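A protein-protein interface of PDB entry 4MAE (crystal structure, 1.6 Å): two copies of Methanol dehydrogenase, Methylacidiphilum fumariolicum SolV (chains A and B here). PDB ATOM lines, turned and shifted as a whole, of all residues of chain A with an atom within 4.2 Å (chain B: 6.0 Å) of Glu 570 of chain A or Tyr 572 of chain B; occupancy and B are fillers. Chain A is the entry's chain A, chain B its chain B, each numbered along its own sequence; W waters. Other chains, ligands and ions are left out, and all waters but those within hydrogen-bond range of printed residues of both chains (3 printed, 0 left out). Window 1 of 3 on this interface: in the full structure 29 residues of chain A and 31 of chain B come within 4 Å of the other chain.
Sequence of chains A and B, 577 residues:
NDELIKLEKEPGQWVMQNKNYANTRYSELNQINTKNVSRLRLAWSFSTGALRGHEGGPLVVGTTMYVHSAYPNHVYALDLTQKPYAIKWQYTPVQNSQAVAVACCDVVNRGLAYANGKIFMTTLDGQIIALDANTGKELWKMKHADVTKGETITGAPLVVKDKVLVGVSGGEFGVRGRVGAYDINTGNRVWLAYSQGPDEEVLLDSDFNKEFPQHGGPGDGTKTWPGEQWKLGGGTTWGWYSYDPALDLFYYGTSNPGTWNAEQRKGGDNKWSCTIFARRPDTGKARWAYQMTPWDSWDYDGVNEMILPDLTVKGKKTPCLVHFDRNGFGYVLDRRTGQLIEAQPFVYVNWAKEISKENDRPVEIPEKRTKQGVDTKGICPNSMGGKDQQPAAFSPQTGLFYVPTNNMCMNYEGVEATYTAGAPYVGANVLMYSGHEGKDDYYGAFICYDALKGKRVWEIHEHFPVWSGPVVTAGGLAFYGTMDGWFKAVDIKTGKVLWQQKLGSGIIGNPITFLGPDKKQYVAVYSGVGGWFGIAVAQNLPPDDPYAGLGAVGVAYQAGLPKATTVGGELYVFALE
The backbone NH of Gly 504 of chain B is in hydrogen-bond range of the side-chain hydroxyl of Ser 45 of chain A. OG of Ser 45 of chain A is in hydrogen-bond range of OH of Tyr 572 of chain B (2.6 Å). The backbone NH of Ser 47 of chain A lies within hydrogen-bond range of the backbone carbonyl oxygen of Gly 504 of chain B (2.9 Å). The side-chain hydroxyl (OG) of Ser 47 of chain A sits at hydrogen-bond distance from the backbone carbonyl oxygen (O) of Val 567 of chain B (2.6 Å). The side-chain hydroxyl (OH) of Tyr 572 of chain A sits at hydrogen-bond distance from the side-chain hydroxyl (OG) of Ser 45 of chain B (2.6 Å). O of Ser 45 of chain A sits close to O of Leu 503 of chain B (3.3 Å). OH of Tyr 572 of chain B lies close to OE2 of Glu 570 of chain A (2.2 Å). OH of Tyr 572 of chain A lies close to OE2 of Glu 570 of chain B, 2.3 Å away.
O of Phe 46 of chain A sits at hydrogen-bond distance from N of Leu 571 of chain A, 2.8 Å away. The side-chain hydroxyl (OG) of Ser 47 of chain A lies close to the side-chain carboxylate (OE1) of Glu 570 of chain A, at 3.4 Å. O of Val 525 of chain A is in hydrogen-bond range of N of Tyr 572 of chain A, 2.9 Å away. N of Ser 527 of chain A sits at hydrogen-bond distance from O of Glu 570 of chain A. N of Tyr 572 of chain B is in hydrogen-bond range of O of Val 525 of chain B (2.9 Å). O of Glu 570 of chain B sits at hydrogen-bond distance from N of Ser 527 of chain B (2.7 Å).
Among the printed residues, merely in contact across the chains: Ser 47 of chain A with Gly 568 of chain B (3.5 Å), Glu 570 of chain A with Gly 504 of chain B (3.5 Å) and Phe 46 of chain A with Gly 504 of chain B (3.6 Å).
Glu 570 of chain A touches just these residues of chain B: Gly 504 and Tyr 572. Of the printed residues of chain A, Gly 504 of chain B touches Ser 45 (3.3 Å), Phe 46 (3.6 Å), Ser 47 (2.9 Å) and Glu 570 (3.5 Å). Ser 527 of chain B touches none of the printed residues of chain A. Of the printed residues of chain A, Gly 568 of chain B touches Ser 47. Tyr 572 of chain B touches two residues of chain A. The nearest residue of chain A that does not touch Tyr 572 of chain B is Tyr 572 of chain A (4.04 Å). The nearest printed residue of chain A that does not touch Leu 503 of chain B is Phe 46 of chain A (4.8 Å).
Of the 21 printed residues of chain B, 7 touch a printed residue of chain A. Of the 10 printed residues of chain A, 5 touch a printed residue of chain B. Hydrophobic or aromatic side chains of chain A that line the printed part of chain B: Tyr 572. Among the printed residues, no Asp or Glu carboxylate lies within 4 Å of a Lys or Arg side-chain nitrogen of the other chain.
Ser 45 of chain A touches Tyr 572 of chain B, and with the chains exchanged Tyr 572 of chain A touches Ser 45 of chain B. Glu 570 of chain A touches Tyr 572 of chain B, and with the chains exchanged Tyr 572 of chain A touches Glu 570 of chain B. 9 positions are printed for both chains.
Water W1 lies within hydrogen-bond range of OG of Ser 527 of chain B (2.9 Å), OE2 of Glu 570 of chain A (2.9 Å) and N of Ser 505 of chain B (3.5 Å). Water W3 bridges NE2 of Gln 501 of chain B and OG of Ser 45 of chain A. Water W2 bridges the side-chain hydroxyl of Ser 527 of chain A (3.0 Å) and the side-chain carboxylate of Glu 570 of chain B (3.0 Å).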
ATOM      1  N   SER A  45     -14.844 -25.870  22.380  1.00  0.00           N
ATOM      2  CA  SER A  45     -16.256 -26.057  22.057  1.00  0.00           C
ATOM      3  C   SER A  45     -16.451 -27.141  21.008  1.00  0.00           C
ATOM      4  O   SER A  45     -15.493 -27.582  20.376  1.00  0.00           O
ATOM      5  CB  SER A  45     -16.896 -24.740  21.601  1.00  0.00           C
ATOM      6  OG  SER A  45     -16.180 -24.171  20.525  1.00  0.00           O
ATOM      7  N   PHE A  46     -17.704 -27.563  20.847  1.00  0.00           N
ATOM      8  CA  PHE A  46     -18.063 -28.684  19.987  1.00  0.00           C
ATOM      9  C   PHE A  46     -19.488 -28.488  19.474  1.00  0.00           C
ATOM     10  O   PHE A  46     -20.401 -28.311  20.272  1.00  0.00           O
ATOM     11  CB  PHE A  46     -17.965 -29.989  20.785  1.00  0.00           C
ATOM     12  CG  PHE A  46     -18.475 -31.190  20.046  1.00  0.00           C
ATOM     13  CD1 PHE A  46     -17.760 -31.711  18.978  1.00  0.00           C
ATOM     14  CD2 PHE A  46     -19.667 -31.801  20.417  1.00  0.00           C
ATOM     15  CE1 PHE A  46     -18.223 -32.813  18.294  1.00  0.00           C
ATOM     16  CE2 PHE A  46     -20.133 -32.911  19.733  1.00  0.00           C
ATOM     17  CZ  PHE A  46     -19.409 -33.412  18.670  1.00  0.00           C
ATOM     18  N   SER A  47     -19.670 -28.510  18.151  1.00  0.00           N
ATOM     19  CA  SER A  47     -20.996 -28.379  17.546  1.00  0.00           C
ATOM     20  C   SER A  47     -21.739 -29.715  17.547  1.00  0.00           C
ATOM     21  O   SER A  47     -21.190 -30.745  17.145  1.00  0.00           O
ATOM     22  CB  SER A  47     -20.889 -27.860  16.104  1.00  0.00           C
ATOM     23  OG  SER A  47     -22.177 -27.672  15.551  1.00  0.00           O
ATOM     24  N   VAL A 525     -21.657 -26.360  29.071  1.00  0.00           N
ATOM     25  CA  VAL A 525     -23.074 -26.059  28.874  1.00  0.00           C
ATOM     26  C   VAL A 525     -23.427 -26.031  27.391  1.00  0.00           C
ATOM     27  O   VAL A 525     -22.603 -25.647  26.568  1.00  0.00           O
ATOM     28  CB  VAL A 525     -23.466 -24.703  29.537  1.00  0.00           C
ATOM     29  CG1 VAL A 525     -22.938 -23.508  28.729  1.00  0.00           C
ATOM     30  CG2 VAL A 525     -24.976 -24.603  29.729  1.00  0.00           C
ATOM     31  N   TYR A 526     -24.643 -26.459  27.065  1.00  0.00           N
ATOM     32  CA  TYR A 526     -25.181 -26.342  25.715  1.00  0.00           C
ATOM     33  C   TYR A 526     -25.733 -24.949  25.473  1.00  0.00           C
ATOM     34  O   TYR A 526     -26.333 -24.357  26.362  1.00  0.00           O
ATOM     35  CB  TYR A 526     -26.357 -27.290  25.504  1.00  0.00           C
ATOM     36  CG  TYR A 526     -26.064 -28.778  25.539  1.00  0.00           C
ATOM     37  CD1 TYR A 526     -27.025 -29.667  26.002  1.00  0.00           C
ATOM     38  CD2 TYR A 526     -24.856 -29.308  25.077  1.00  0.00           C
ATOM     39  CE1 TYR A 526     -26.799 -31.023  26.024  1.00  0.00           C
ATOM     40  CE2 TYR A 526     -24.619 -30.676  25.103  1.00  0.00           C
ATOM     41  CZ  TYR A 526     -25.597 -31.531  25.580  1.00  0.00           C
ATOM     42  OH  TYR A 526     -25.393 -32.896  25.600  1.00  0.00           O
ATOM     43  N   SER A 527     -25.578 -24.475  24.241  1.00  0.00           N
ATOM     44  CA  SER A 527     -26.257 -23.297  23.729  1.00  0.00           C
ATOM     45  C   SER A 527     -27.106 -23.756  22.542  1.00  0.00           C
ATOM     46  O   SER A 527     -26.692 -24.628  21.779  1.00  0.00           O
ATOM     47  CB  SER A 527     -25.218 -22.258  23.294  1.00  0.00           C
ATOM     48  OG  SER A 527     -25.748 -21.304  22.409  1.00  0.00           O
ATOM     49  N   GLY A 569     -26.785 -24.859  18.197  1.00  0.00           N
ATOM     50  CA  GLY A 569     -26.550 -26.138  18.848  1.00  0.00           C
ATOM     51  C   GLY A 569     -25.064 -26.315  19.049  1.00  0.00           C
ATOM     52  O   GLY A 569     -24.369 -26.865  18.190  1.00  0.00           O
ATOM     53  N   GLU A 570     -24.573 -25.817  20.180  1.00  0.00           N
ATOM     54  CA  GLU A 570     -23.149 -25.787  20.448  1.00  0.00           C
ATOM     55  C   GLU A 570     -22.892 -26.114  21.909  1.00  0.00           C
ATOM     56  O   GLU A 570     -23.603 -25.642  22.794  1.00  0.00           O
ATOM     57  CB  GLU A 570     -22.590 -24.395  20.140  1.00  0.00           C
ATOM     58  CG  GLU A 570     -21.080 -24.348  19.935  1.00  0.00           C
ATOM     59  CD  GLU A 570     -20.668 -24.540  18.492  1.00  0.00           C
ATOM     60  OE1 GLU A 570     -21.465 -25.097  17.707  1.00  0.00           O
ATOM     61  OE2 GLU A 570     -19.541 -24.140  18.150  1.00  0.00           O
ATOM     62  N   LEU A 571     -21.871 -26.921  22.145  1.00  0.00           N
ATOM     63  CA  LEU A 571     -21.404 -27.220  23.493  1.00  0.00           C
ATOM     64  C   LEU A 571     -20.189 -26.341  23.762  1.00  0.00           C
ATOM     65  O   LEU A 571     -19.228 -26.374  22.997  1.00  0.00           O
ATOM     66  CB  LEU A 571     -21.036 -28.701  23.602  1.00  0.00           C
ATOM     67  CG  LEU A 571     -20.290 -29.143  24.862  1.00  0.00           C
ATOM     68  CD1 LEU A 571     -21.174 -28.943  26.074  1.00  0.00           C
ATOM     69  CD2 LEU A 571     -19.834 -30.586  24.744  1.00  0.00           C
ATOM     70  N   TYR A 572     -20.256 -25.545  24.833  1.00  0.00           N
ATOM     71  CA  TYR A 572     -19.168 -24.651  25.257  1.00  0.00           C
ATOM     72  C   TYR A 572     -18.565 -25.133  26.577  1.00  0.00           C
ATOM     73  O   TYR A 572     -19.303 -25.409  27.535  1.00  0.00           O
ATOM     74  CB  TYR A 572     -19.715 -23.244  25.479  1.00  0.00           C
ATOM     75  CG  TYR A 572     -20.022 -22.460  24.222  1.00  0.00           C
ATOM     76  CD1 TYR A 572     -19.068 -21.611  23.668  1.00  0.00           C
ATOM     77  CD2 TYR A 572     -21.269 -22.525  23.616  1.00  0.00           C
ATOM     78  CE1 TYR A 572     -19.333 -20.864  22.531  1.00  0.00           C
ATOM     79  CE2 TYR A 572     -21.545 -21.777  22.465  1.00  0.00           C
ATOM     80  CZ  TYR A 572     -20.568 -20.948  21.934  1.00  0.00           C
ATOM     81  OH  TYR A 572     -20.799 -20.191  20.800  1.00  0.00           O
ATOM     82  N   LEU B  42     -11.745 -16.194  23.814  1.00  0.00           N
ATOM     83  CA  LEU B  42     -13.035 -15.875  23.236  1.00  0.00           C
ATOM     84  C   LEU B  42     -13.676 -14.730  24.009  1.00  0.00           C
ATOM     85  O   LEU B  42     -13.704 -14.753  25.247  1.00  0.00           O
ATOM     86  CB  LEU B  42     -13.964 -17.090  23.258  1.00  0.00           C
ATOM     87  CG  LEU B  42     -15.293 -16.905  22.516  1.00  0.00           C
ATOM     88  CD1 LEU B  42     -15.061 -16.741  21.024  1.00  0.00           C
ATOM     89  CD2 LEU B  42     -16.199 -18.097  22.788  1.00  0.00           C
ATOM     90  N   TRP B  44     -16.890 -13.213  22.614  1.00  0.00           N
ATOM     91  CA  TRP B  44     -18.303 -13.505  22.423  1.00  0.00           C
ATOM     92  C   TRP B  44     -18.499 -14.338  21.168  1.00  0.00           C
ATOM     93  O   TRP B  44     -17.577 -14.486  20.371  1.00  0.00           O
ATOM     94  CB  TRP B  44     -19.129 -12.219  22.320  1.00  0.00           C
ATOM     95  CG  TRP B  44     -18.709 -11.193  21.271  1.00  0.00           C
ATOM     96  CD1 TRP B  44     -17.849 -10.150  21.449  1.00  0.00           C
ATOM     97  CD2 TRP B  44     -19.215 -11.066  19.933  1.00  0.00           C
ATOM     98  NE1 TRP B  44     -17.755  -9.405  20.295  1.00  0.00           N
ATOM     99  CE2 TRP B  44     -18.591  -9.941  19.353  1.00  0.00           C
ATOM    100  CE3 TRP B  44     -20.120 -11.805  19.162  1.00  0.00           C
ATOM    101  CZ2 TRP B  44     -18.849  -9.534  18.046  1.00  0.00           C
ATOM    102  CZ3 TRP B  44     -20.378 -11.403  17.873  1.00  0.00           C
ATOM    103  CH2 TRP B  44     -19.751 -10.279  17.324  1.00  0.00           C
ATOM    104  N   SER B  45     -19.700 -14.884  21.004  1.00  0.00           N
ATOM    105  CA  SER B  45     -20.040 -15.612  19.781  1.00  0.00           C
ATOM    106  C   SER B  45     -21.496 -15.402  19.399  1.00  0.00           C
ATOM    107  O   SER B  45     -22.279 -14.858  20.179  1.00  0.00           O
ATOM    108  CB  SER B  45     -19.725 -17.103  19.938  1.00  0.00           C
ATOM    109  OG  SER B  45     -20.341 -17.645  21.100  1.00  0.00           O
ATOM    110  N   PHE B  46     -21.836 -15.846  18.192  1.00  0.00           N
ATOM    111  CA  PHE B  46     -23.139 -15.618  17.599  1.00  0.00           C
ATOM    112  C   PHE B  46     -23.427 -16.756  16.625  1.00  0.00           C
ATOM    113  O   PHE B  46     -22.649 -17.004  15.715  1.00  0.00           O
ATOM    114  CB  PHE B  46     -23.147 -14.269  16.875  1.00  0.00           C
ATOM    115  CG  PHE B  46     -24.385 -14.012  16.085  1.00  0.00           C
ATOM    116  CD1 PHE B  46     -25.593 -13.787  16.727  1.00  0.00           C
ATOM    117  CD2 PHE B  46     -24.356 -14.012  14.698  1.00  0.00           C
ATOM    118  CE1 PHE B  46     -26.744 -13.565  16.002  1.00  0.00           C
ATOM    119  CE2 PHE B  46     -25.506 -13.786  13.974  1.00  0.00           C
ATOM    120  CZ  PHE B  46     -26.699 -13.566  14.625  1.00  0.00           C
ATOM    121  N   GLN B 501      -6.836 -22.564  19.461  1.00  0.00           N
ATOM    122  CA  GLN B 501      -7.986 -23.015  20.236  1.00  0.00           C
ATOM    123  C   GLN B 501      -8.888 -23.854  19.356  1.00  0.00           C
ATOM    124  O   GLN B 501      -9.084 -23.522  18.195  1.00  0.00           O
ATOM    125  CB  GLN B 501      -8.766 -21.819  20.767  1.00  0.00           C
ATOM    126  CG  GLN B 501      -9.947 -22.185  21.652  1.00  0.00           C
ATOM    127  CD  GLN B 501     -10.549 -20.985  22.355  1.00  0.00           C
ATOM    128  OE1 GLN B 501      -9.842 -20.041  22.712  1.00  0.00           O
ATOM    129  NE2 GLN B 501     -11.870 -21.010  22.545  1.00  0.00           N
ATOM    130  N   LEU B 503     -12.378 -25.109  18.130  1.00  0.00           N
ATOM    131  CA  LEU B 503     -13.750 -24.616  18.068  1.00  0.00           C
ATOM    132  C   LEU B 503     -14.681 -25.752  17.646  1.00  0.00           C
ATOM    133  O   LEU B 503     -14.235 -26.882  17.458  1.00  0.00           O
ATOM    134  CB  LEU B 503     -13.844 -23.439  17.091  1.00  0.00           C
ATOM    135  CG  LEU B 503     -12.837 -22.295  17.286  1.00  0.00           C
ATOM    136  CD1 LEU B 503     -13.141 -21.142  16.319  1.00  0.00           C
ATOM    137  CD2 LEU B 503     -12.855 -21.824  18.719  1.00  0.00           C
ATOM    138  N   GLY B 504     -15.966 -25.437  17.481  1.00  0.00           N
ATOM    139  CA  GLY B 504     -17.004 -26.460  17.399  1.00  0.00           C
ATOM    140  C   GLY B 504     -17.134 -27.240  16.100  1.00  0.00           C
ATOM    141  O   GLY B 504     -17.674 -28.355  16.098  1.00  0.00           O
ATOM    142  N   SER B 505     -16.653 -26.656  15.005  1.00  0.00           N
ATOM    143  CA  SER B 505     -16.747 -27.256  13.681  1.00  0.00           C
ATOM    144  C   SER B 505     -15.561 -26.790  12.845  1.00  0.00           C
ATOM    145  O   SER B 505     -14.996 -25.727  13.098  1.00  0.00           O
ATOM    146  CB  SER B 505     -18.060 -26.836  13.002  1.00  0.00           C
ATOM    147  OG  SER B 505     -18.246 -27.486  11.757  1.00  0.00           O
ATOM    148  N   VAL B 523     -10.658 -10.342  16.820  1.00  0.00           N
ATOM    149  CA  VAL B 523     -10.476 -11.225  15.665  1.00  0.00           C
ATOM    150  C   VAL B 523     -11.700 -12.138  15.584  1.00  0.00           C
ATOM    151  O   VAL B 523     -12.055 -12.779  16.571  1.00  0.00           O
ATOM    152  CB  VAL B 523      -9.176 -12.054  15.773  1.00  0.00           C
ATOM    153  CG1 VAL B 523      -9.037 -12.997  14.571  1.00  0.00           C
ATOM    154  CG2 VAL B 523      -7.966 -11.128  15.882  1.00  0.00           C
ATOM    155  N   ALA B 524     -12.345 -12.182  14.414  1.00  0.00           N
ATOM    156  CA  ALA B 524     -13.602 -12.921  14.240  1.00  0.00           C
ATOM    157  C   ALA B 524     -13.499 -13.910  13.092  1.00  0.00           C
ATOM    158  O   ALA B 524     -12.891 -13.607  12.068  1.00  0.00           O
ATOM    159  CB  ALA B 524     -14.758 -11.948  13.998  1.00  0.00           C
ATOM    160  N   VAL B 525     -14.095 -15.089  13.268  1.00  0.00           N
ATOM    161  CA  VAL B 525     -14.085 -16.134  12.233  1.00  0.00           C
ATOM    162  C   VAL B 525     -15.318 -17.025  12.332  1.00  0.00           C
ATOM    163  O   VAL B 525     -15.811 -17.310  13.432  1.00  0.00           O
ATOM    164  CB  VAL B 525     -12.793 -17.005  12.318  1.00  0.00           C
ATOM    165  CG1 VAL B 525     -12.828 -17.943  13.524  1.00  0.00           C
ATOM    166  CG2 VAL B 525     -12.560 -17.791  11.019  1.00  0.00           C
ATOM    167  N   TYR B 526     -15.823 -17.452  11.176  1.00  0.00           N
ATOM    168  CA  TYR B 526     -16.902 -18.435  11.129  1.00  0.00           C
ATOM    169  C   TYR B 526     -16.344 -19.830  11.363  1.00  0.00           C
ATOM    170  O   TYR B 526     -15.269 -20.166  10.865  1.00  0.00           O
ATOM    171  CB  TYR B 526     -17.582 -18.471   9.761  1.00  0.00           C
ATOM    172  CG  TYR B 526     -18.323 -17.236   9.319  1.00  0.00           C
ATOM    173  CD1 TYR B 526     -18.340 -16.867   7.982  1.00  0.00           C
ATOM    174  CD2 TYR B 526     -19.034 -16.450  10.219  1.00  0.00           C
ATOM    175  CE1 TYR B 526     -19.035 -15.748   7.556  1.00  0.00           C
ATOM    176  CE2 TYR B 526     -19.726 -15.325   9.799  1.00  0.00           C
ATOM    177  CZ  TYR B 526     -19.731 -14.982   8.462  1.00  0.00           C
ATOM    178  OH  TYR B 526     -20.411 -13.858   8.046  1.00  0.00           O
ATOM    179  N   SER B 527     -17.108 -20.633  12.096  1.00  0.00           N
ATOM    180  CA  SER B 527     -16.913 -22.068  12.205  1.00  0.00           C
ATOM    181  C   SER B 527     -18.153 -22.753  11.602  1.00  0.00           C
ATOM    182  O   SER B 527     -19.281 -22.257  11.728  1.00  0.00           O
ATOM    183  CB  SER B 527     -16.694 -22.428  13.686  1.00  0.00           C
ATOM    184  OG  SER B 527     -16.966 -23.779  13.970  1.00  0.00           O
ATOM    185  N   VAL B 567     -21.021 -30.758  11.561  1.00  0.00           N
ATOM    186  CA  VAL B 567     -21.487 -29.517  10.953  1.00  0.00           C
ATOM    187  C   VAL B 567     -21.846 -28.482  12.007  1.00  0.00           C
ATOM    188  O   VAL B 567     -22.107 -28.802  13.182  1.00  0.00           O
ATOM    189  CB  VAL B 567     -22.688 -29.722  10.001  1.00  0.00           C
ATOM    190  CG1 VAL B 567     -22.297 -30.629   8.842  1.00  0.00           C
ATOM    191  CG2 VAL B 567     -23.907 -30.276  10.751  1.00  0.00           C
ATOM    192  N   GLY B 568     -21.869 -27.233  11.566  1.00  0.00           N
ATOM    193  CA  GLY B 568     -22.155 -26.121  12.439  1.00  0.00           C
ATOM    194  C   GLY B 568     -22.329 -24.820  11.683  1.00  0.00           C
ATOM    195  O   GLY B 568     -22.420 -24.801  10.448  1.00  0.00           O
ATOM    196  N   GLY B 569     -22.389 -23.734  12.444  1.00  0.00           N
ATOM    197  CA  GLY B 569     -22.546 -22.397  11.888  1.00  0.00           C
ATOM    198  C   GLY B 569     -22.537 -21.396  13.016  1.00  0.00           C
ATOM    199  O   GLY B 569     -23.590 -21.023  13.519  1.00  0.00           O
ATOM    200  N   GLU B 570     -21.331 -20.972  13.401  1.00  0.00           N
ATOM    201  CA  GLU B 570     -21.115 -20.152  14.577  1.00  0.00           C
ATOM    202  C   GLU B 570     -20.026 -19.132  14.281  1.00  0.00           C
ATOM    203  O   GLU B 570     -18.999 -19.462  13.683  1.00  0.00           O
ATOM    204  CB  GLU B 570     -20.688 -21.046  15.750  1.00  0.00           C
ATOM    205  CG  GLU B 570     -20.767 -20.399  17.128  1.00  0.00           C
ATOM    206  CD  GLU B 570     -22.114 -20.587  17.796  1.00  0.00           C
ATOM    207  OE1 GLU B 570     -23.095 -20.868  17.087  1.00  0.00           O
ATOM    208  OE2 GLU B 570     -22.189 -20.450  19.029  1.00  0.00           O
ATOM    209  N   LEU B 571     -20.270 -17.888  14.666  1.00  0.00           N
ATOM    210  CA  LEU B 571     -19.265 -16.833  14.566  1.00  0.00           C
ATOM    211  C   LEU B 571     -18.591 -16.702  15.932  1.00  0.00           C
ATOM    212  O   LEU B 571     -19.256 -16.457  16.940  1.00  0.00           O
ATOM    213  CB  LEU B 571     -19.901 -15.502  14.146  1.00  0.00           C
ATOM    214  CG  LEU B 571     -19.025 -14.249  14.247  1.00  0.00           C
ATOM    215  CD1 LEU B 571     -17.882 -14.306  13.244  1.00  0.00           C
ATOM    216  CD2 LEU B 571     -19.896 -13.027  14.024  1.00  0.00           C
ATOM    217  N   TYR B 572     -17.272 -16.883  15.948  1.00  0.00           N
ATOM    218  CA  TYR B 572     -16.468 -16.763  17.157  1.00  0.00           C
ATOM    219  C   TYR B 572     -15.638 -15.478  17.097  1.00  0.00           C
ATOM    220  O   TYR B 572     -14.967 -15.217  16.100  1.00  0.00           O
ATOM    221  CB  TYR B 572     -15.530 -17.966  17.273  1.00  0.00           C
ATOM    222  CG  TYR B 572     -16.185 -19.271  17.698  1.00  0.00           C
ATOM    223  CD1 TYR B 572     -16.173 -19.663  19.028  1.00  0.00           C
ATOM    224  CD2 TYR B 572     -16.766 -20.135  16.772  1.00  0.00           C
ATOM    225  CE1 TYR B 572     -16.739 -20.852  19.439  1.00  0.00           C
ATOM    226  CE2 TYR B 572     -17.351 -21.341  17.185  1.00  0.00           C
ATOM    227  CZ  TYR B 572     -17.329 -21.687  18.524  1.00  0.00           C
ATOM    228  OH  TYR B 572     -17.883 -22.877  18.974  1.00  0.00           O
ATOM    229  N   VAL B 573     -15.676 -14.688  18.166  1.00  0.00           N
ATOM    230  CA  VAL B 573     -14.965 -13.413  18.216  1.00  0.00           C
ATOM    231  C   VAL B 573     -14.019 -13.373  19.420  1.00  0.00           C
ATOM    232  O   VAL B 573     -14.452 -13.544  20.560  1.00  0.00           O
ATOM    233  CB  VAL B 573     -15.961 -12.248  18.277  1.00  0.00           C
ATOM    234  CG1 VAL B 573     -15.241 -10.909  18.214  1.00  0.00           C
ATOM    235  CG2 VAL B 573     -16.964 -12.372  17.126  1.00  0.00           C
ATOM    236  N   PHE B 574     -12.735 -13.136  19.158  1.00  0.00           N
ATOM    237  CA  PHE B 574     -11.685 -13.226  20.174  1.00  0.00           C
ATOM    238  C   PHE B 574     -11.072 -11.861  20.472  1.00  0.00           C
ATOM    239  O   PHE B 574     -11.047 -10.987  19.606  1.00  0.00           O
ATOM    240  CB  PHE B 574     -10.563 -14.162  19.701  1.00  0.00           C
ATOM    241  CG  PHE B 574     -11.008 -15.576  19.456  1.00  0.00           C
ATOM    242  CD1 PHE B 574     -11.595 -15.943  18.242  1.00  0.00           C
ATOM    243  CD2 PHE B 574     -10.857 -16.541  20.436  1.00  0.00           C
ATOM    244  CE1 PHE B 574     -12.024 -17.268  18.020  1.00  0.00           C
ATOM    245  CE2 PHE B 574     -11.276 -17.860  20.221  1.00  0.00           C
ATOM    246  CZ  PHE B 574     -11.864 -18.220  19.014  1.00  0.00           C
HETATM  247  O   HOH W   1     -19.379 -24.499  15.316  1.00  0.00           O
HETATM  248  O   HOH W   2     -24.930 -21.677  19.542  1.00  0.00           O
HETATM  249  O   HOH W   3     -13.526 -23.238  21.524  1.00  0.00           O
